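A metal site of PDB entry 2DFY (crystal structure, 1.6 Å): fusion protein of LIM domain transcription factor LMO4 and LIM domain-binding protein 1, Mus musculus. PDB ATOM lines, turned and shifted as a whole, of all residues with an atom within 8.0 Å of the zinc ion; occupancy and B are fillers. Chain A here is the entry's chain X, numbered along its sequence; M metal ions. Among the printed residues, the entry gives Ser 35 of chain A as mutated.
Within 4 Å of the zinc ion: Cys 33, Cys 36, Cys 56 and Asp 59.
Along chain A the residues within 4 Å of the zinc ion span positions 33 to 59.
The nearest printed residue that does not touch the zinc ion is Ser 35 (4.6 Å).
The zinc ion is bound by the side-chain carboxylate (OD2) of Asp 59 (2.1 Å), the side-chain sulfur (SG) of Cys 36 (2.3 Å), the side-chain sulfur (SG) of Cys 56 (2.3 Å) and the side-chain sulfur (SG) of Cys 33 (2.3 Å).
The zinc ion has four donor atoms within binding distance.
The side-chain carboxylate (OD1) of Asp 59 lies within salt-bridge range of the guanidinium group (NE) of Arg 62 (2.9 Å).
The backbone NH (N) of Ser 35 sits close to the side-chain sulfur (SG) of Cys 33.
O of Ala 38 lies within hydrogen-bond range of N of Cys 33 (2.9 Å).
SG of Cys 36 lies close to N of Ala 38, at 3.5 Å.
SG of Cys 56 lies close to N of Asn 58 (3.7 Å).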
ATOM      1  N   LYS A  32      23.893 -33.203  19.180  1.00  0.00           N
ATOM      2  CA  LYS A  32      22.592 -33.466  19.712  1.00  0.00           C
ATOM      3  C   LYS A  32      22.450 -32.928  21.127  1.00  0.00           C
ATOM      4  O   LYS A  32      23.455 -32.813  21.847  1.00  0.00           O
ATOM      5  CB  LYS A  32      22.370 -34.966  19.761  1.00  0.00           C
ATOM      6  CG  LYS A  32      22.252 -35.631  18.466  1.00  0.00           C
ATOM      7  CD  LYS A  32      22.086 -37.184  18.689  1.00  0.00           C
ATOM      8  CE  LYS A  32      23.306 -37.904  19.177  1.00  0.00           C
ATOM      9  NZ  LYS A  32      23.074 -39.441  19.202  1.00  0.00           N
ATOM     10  N   CYS A  33      21.244 -32.534  21.466  1.00  0.00           N
ATOM     11  CA  CYS A  33      20.951 -32.066  22.830  1.00  0.00           C
ATOM     12  C   CYS A  33      21.142 -33.196  23.805  1.00  0.00           C
ATOM     13  O   CYS A  33      20.602 -34.269  23.595  1.00  0.00           O
ATOM     14  CB  CYS A  33      19.520 -31.616  22.974  1.00  0.00           C
ATOM     15  SG  CYS A  33      19.093 -31.008  24.643  1.00  0.00           S
ATOM     16  N   SER A  34      21.884 -32.949  24.905  1.00  0.00           N
ATOM     17  CA  SER A  34      22.094 -34.012  25.912  1.00  0.00           C
ATOM     18  C   SER A  34      20.770 -34.498  26.503  1.00  0.00           C
ATOM     19  O   SER A  34      20.642 -35.698  26.842  1.00  0.00           O
ATOM     20  CB  SER A  34      23.039 -33.528  27.032  1.00  0.00           C
ATOM     21  OG  SER A  34      24.308 -33.061  26.578  1.00  0.00           O
ATOM     22  N   SER A  35      19.791 -33.610  26.652  1.00  0.00           N
ATOM     23  CA  SER A  35      18.541 -33.948  27.331  1.00  0.00           C
ATOM     24  C   SER A  35      17.531 -34.607  26.388  1.00  0.00           C
ATOM     25  O   SER A  35      16.995 -35.679  26.715  1.00  0.00           O
ATOM     26  CB  SER A  35      17.924 -32.727  27.969  1.00  0.00           C
ATOM     27  OG  SER A  35      16.676 -33.034  28.582  1.00  0.00           O
ATOM     28  N   CYS A  36      17.304 -33.991  25.218  1.00  0.00           N
ATOM     29  CA  CYS A  36      16.173 -34.433  24.346  1.00  0.00           C
ATOM     30  C   CYS A  36      16.625 -35.091  23.048  1.00  0.00           C
ATOM     31  O   CYS A  36      15.773 -35.552  22.259  1.00  0.00           O
ATOM     32  CB  CYS A  36      15.255 -33.249  24.079  1.00  0.00           C
ATOM     33  SG  CYS A  36      15.888 -32.088  22.857  1.00  0.00           S
ATOM     34  N   GLN A  37      17.953 -35.129  22.808  1.00  0.00           N
ATOM     35  CA  GLN A  37      18.542 -35.698  21.604  1.00  0.00           C
ATOM     36  C   GLN A  37      18.190 -34.972  20.266  1.00  0.00           C
ATOM     37  O   GLN A  37      18.487 -35.499  19.185  1.00  0.00           O
ATOM     38  CB  GLN A  37      18.277 -37.209  21.492  1.00  0.00           C
ATOM     39  CG  GLN A  37      18.895 -38.020  22.581  1.00  0.00           C
ATOM     40  CD  GLN A  37      18.226 -37.839  23.904  1.00  0.00           C
ATOM     41  OE1 GLN A  37      17.002 -38.020  24.051  1.00  0.00           O
ATOM     42  NE2 GLN A  37      19.018 -37.481  24.921  1.00  0.00           N
ATOM     43  N   ALA A  38      17.638 -33.768  20.364  1.00  0.00           N
ATOM     44  CA  ALA A  38      17.335 -32.988  19.116  1.00  0.00           C
ATOM     45  C   ALA A  38      18.627 -32.723  18.363  1.00  0.00           C
ATOM     46  O   ALA A  38      19.713 -32.508  18.998  1.00  0.00           O
ATOM     47  CB  ALA A  38      16.679 -31.691  19.443  1.00  0.00           C
ATOM     48  N   GLN A  39      18.527 -32.708  17.024  1.00  0.00           N
ATOM     49  CA  GLN A  39      19.663 -32.400  16.176  1.00  0.00           C
ATOM     50  C   GLN A  39      19.792 -30.870  16.121  1.00  0.00           C
ATOM     51  O   GLN A  39      19.028 -30.183  15.427  1.00  0.00           O
ATOM     52  CB  GLN A  39      19.501 -33.036  14.788  1.00  0.00           C
ATOM     53  CG  GLN A  39      19.740 -34.555  14.851  1.00  0.00           C
ATOM     54  CD  GLN A  39      19.761 -35.193  13.482  1.00  0.00           C
ATOM     55  OE1 GLN A  39      19.570 -34.510  12.513  1.00  0.00           O
ATOM     56  NE2 GLN A  39      20.111 -36.424  13.399  1.00  0.00           N
ATOM     57  N   LEU A  40      20.706 -30.338  16.945  1.00  0.00           N
ATOM     58  CA  LEU A  40      20.806 -28.908  17.200  1.00  0.00           C
ATOM     59  C   LEU A  40      20.950 -28.050  15.940  1.00  0.00           C
ATOM     60  O   LEU A  40      20.412 -26.958  15.894  1.00  0.00           O
ATOM     61  CB  LEU A  40      21.962 -28.622  18.168  1.00  0.00           C
ATOM     62  CG  LEU A  40      21.746 -29.238  19.530  1.00  0.00           C
ATOM     63  CD1 LEU A  40      22.925 -28.900  20.467  1.00  0.00           C
ATOM     64  CD2 LEU A  40      20.479 -28.837  20.138  1.00  0.00           C
ATOM     65  N   ILE A  43      17.326 -27.819  14.347  1.00  0.00           N
ATOM     66  CA  ILE A  43      16.240 -27.235  15.093  1.00  0.00           C
ATOM     67  C   ILE A  43      16.342 -25.751  15.323  1.00  0.00           C
ATOM     68  O   ILE A  43      15.312 -25.095  15.395  1.00  0.00           O
ATOM     69  CB  ILE A  43      15.899 -28.031  16.381  1.00  0.00           C
ATOM     70  CG1 ILE A  43      17.040 -28.006  17.354  1.00  0.00           C
ATOM     71  CG2 ILE A  43      15.606 -29.437  16.051  1.00  0.00           C
ATOM     72  CD1 ILE A  43      16.559 -28.097  18.739  1.00  0.00           C
ATOM     73  N   ILE A  54      25.519 -30.327  26.474  1.00  0.00           N
ATOM     74  CA  ILE A  54      25.309 -29.491  25.319  1.00  0.00           C
ATOM     75  C   ILE A  54      23.812 -29.539  25.087  1.00  0.00           C
ATOM     76  O   ILE A  54      23.253 -30.616  24.891  1.00  0.00           O
ATOM     77  CB  ILE A  54      26.066 -30.010  24.085  1.00  0.00           C
ATOM     78  CG1 ILE A  54      27.593 -29.913  24.281  1.00  0.00           C
ATOM     79  CG2 ILE A  54      25.635 -29.238  22.911  1.00  0.00           C
ATOM     80  CD1 ILE A  54      28.356 -30.583  23.251  1.00  0.00           C
ATOM     81  N   LEU A  55      23.153 -28.385  25.188  1.00  0.00           N
ATOM     82  CA  LEU A  55      21.684 -28.305  25.254  1.00  0.00           C
ATOM     83  C   LEU A  55      21.060 -27.436  24.144  1.00  0.00           C
ATOM     84  O   LEU A  55      21.644 -26.447  23.698  1.00  0.00           O
ATOM     85  CB  LEU A  55      21.248 -27.710  26.591  1.00  0.00           C
ATOM     86  CG  LEU A  55      21.644 -28.577  27.817  1.00  0.00           C
ATOM     87  CD1 LEU A  55      21.430 -27.821  29.067  1.00  0.00           C
ATOM     88  CD2 LEU A  55      20.957 -29.883  27.851  1.00  0.00           C
ATOM     89  N   CYS A  56      19.853 -27.843  23.739  1.00  0.00           N
ATOM     90  CA  CYS A  56      18.982 -26.946  22.959  1.00  0.00           C
ATOM     91  C   CYS A  56      18.515 -25.824  23.840  1.00  0.00           C
ATOM     92  O   CYS A  56      18.613 -25.867  25.098  1.00  0.00           O
ATOM     93  CB  CYS A  56      17.786 -27.700  22.367  1.00  0.00           C
ATOM     94  SG  CYS A  56      16.510 -28.247  23.540  1.00  0.00           S
ATOM     95  N   ARG A  57      18.017 -24.758  23.203  1.00  0.00           N
ATOM     96  CA  ARG A  57      17.504 -23.613  23.950  1.00  0.00           C
ATOM     97  C   ARG A  57      16.453 -24.015  24.974  1.00  0.00           C
ATOM     98  O   ARG A  57      16.511 -23.599  26.130  1.00  0.00           O
ATOM     99  CB  ARG A  57      16.889 -22.604  22.976  1.00  0.00           C
ATOM    100  CG  ARG A  57      16.278 -21.388  23.671  1.00  0.00           C
ATOM    101  CD  ARG A  57      16.041 -20.219  22.671  1.00  0.00           C
ATOM    102  NE  ARG A  57      17.327 -19.730  22.141  1.00  0.00           N
ATOM    103  CZ  ARG A  57      17.500 -19.022  21.017  1.00  0.00           C
ATOM    104  NH1 ARG A  57      16.464 -18.708  20.235  1.00  0.00           N
ATOM    105  NH2 ARG A  57      18.722 -18.637  20.666  1.00  0.00           N
ATOM    106  N   ASN A  58      15.495 -24.822  24.551  1.00  0.00           N
ATOM    107  CA  ASN A  58      14.354 -25.179  25.416  1.00  0.00           C
ATOM    108  C   ASN A  58      14.828 -25.944  26.672  1.00  0.00           C
ATOM    109  O   ASN A  58      14.398 -25.643  27.786  1.00  0.00           O
ATOM    110  CB  ASN A  58      13.322 -25.957  24.669  1.00  0.00           C
ATOM    111  CG  ASN A  58      12.540 -25.109  23.682  1.00  0.00           C
ATOM    112  OD1 ASN A  58      12.449 -23.877  23.816  1.00  0.00           O
ATOM    113  ND2 ASN A  58      11.944 -25.765  22.682  1.00  0.00           N
ATOM    114  N   ASP A  59      15.764 -26.880  26.498  1.00  0.00           N
ATOM    115  CA  ASP A  59      16.261 -27.616  27.682  1.00  0.00           C
ATOM    116  C   ASP A  59      17.210 -26.791  28.544  1.00  0.00           C
ATOM    117  O   ASP A  59      17.318 -26.990  29.752  1.00  0.00           O
ATOM    118  CB  ASP A  59      16.844 -28.949  27.272  1.00  0.00           C
ATOM    119  CG  ASP A  59      15.745 -29.979  26.974  1.00  0.00           C
ATOM    120  OD1 ASP A  59      14.797 -30.116  27.799  1.00  0.00           O
ATOM    121  OD2 ASP A  59      15.785 -30.625  25.931  1.00  0.00           O
ATOM    122  N   TYR A  60      17.916 -25.846  27.938  1.00  0.00           N
ATOM    123  CA  TYR A  60      18.757 -24.962  28.704  1.00  0.00           C
ATOM    124  C   TYR A  60      17.867 -24.103  29.612  1.00  0.00           C
ATOM    125  O   TYR A  60      18.134 -23.966  30.808  1.00  0.00           O
ATOM    126  CB  TYR A  60      19.596 -24.063  27.810  1.00  0.00           C
ATOM    127  CG  TYR A  60      20.434 -23.056  28.564  1.00  0.00           C
ATOM    128  CD1 TYR A  60      21.598 -23.402  29.206  1.00  0.00           C
ATOM    129  CD2 TYR A  60      20.057 -21.700  28.617  1.00  0.00           C
ATOM    130  CE1 TYR A  60      22.385 -22.463  29.900  1.00  0.00           C
ATOM    131  CE2 TYR A  60      20.837 -20.779  29.275  1.00  0.00           C
ATOM    132  CZ  TYR A  60      21.997 -21.144  29.905  1.00  0.00           C
ATOM    133  OH  TYR A  60      22.764 -20.172  30.540  1.00  0.00           O
ATOM    134  N   ARG A  62      14.829 -24.833  30.608  1.00  0.00           N
ATOM    135  CA  ARG A  62      14.136 -25.712  31.546  1.00  0.00           C
ATOM    136  C   ARG A  62      15.035 -26.066  32.707  1.00  0.00           C
ATOM    137  O   ARG A  62      14.604 -26.077  33.874  1.00  0.00           O
ATOM    138  CB  ARG A  62      13.730 -26.979  30.854  1.00  0.00           C
ATOM    139  CG  ARG A  62      12.971 -27.974  31.712  1.00  0.00           C
ATOM    140  CD  ARG A  62      12.506 -29.163  30.940  1.00  0.00           C
ATOM    141  NE  ARG A  62      13.602 -30.004  30.459  1.00  0.00           N
ATOM    142  CZ  ARG A  62      14.239 -30.926  31.165  1.00  0.00           C
ATOM    143  NH1 ARG A  62      13.912 -31.150  32.457  1.00  0.00           N
ATOM    144  NH2 ARG A  62      15.214 -31.624  30.614  1.00  0.00           N
ATOM    145  N   LEU A  63      16.297 -26.397  32.399  1.00  0.00           N
ATOM    146  CA  LEU A  63      17.222 -26.878  33.425  1.00  0.00           C
ATOM    147  C   LEU A  63      17.906 -25.767  34.216  1.00  0.00           C
ATOM    148  O   LEU A  63      18.253 -25.937  35.400  1.00  0.00           O
ATOM    149  CB  LEU A  63      18.271 -27.808  32.806  1.00  0.00           C
ATOM    150  CG  LEU A  63      17.751 -29.165  32.326  1.00  0.00           C
ATOM    151  CD1 LEU A  63      18.822 -29.935  31.577  1.00  0.00           C
ATOM    152  CD2 LEU A  63      17.219 -29.990  33.527  1.00  0.00           C
HETATM  153 ZN    ZN M   1      16.864 -30.461  24.157  1.00  0.00          ZN
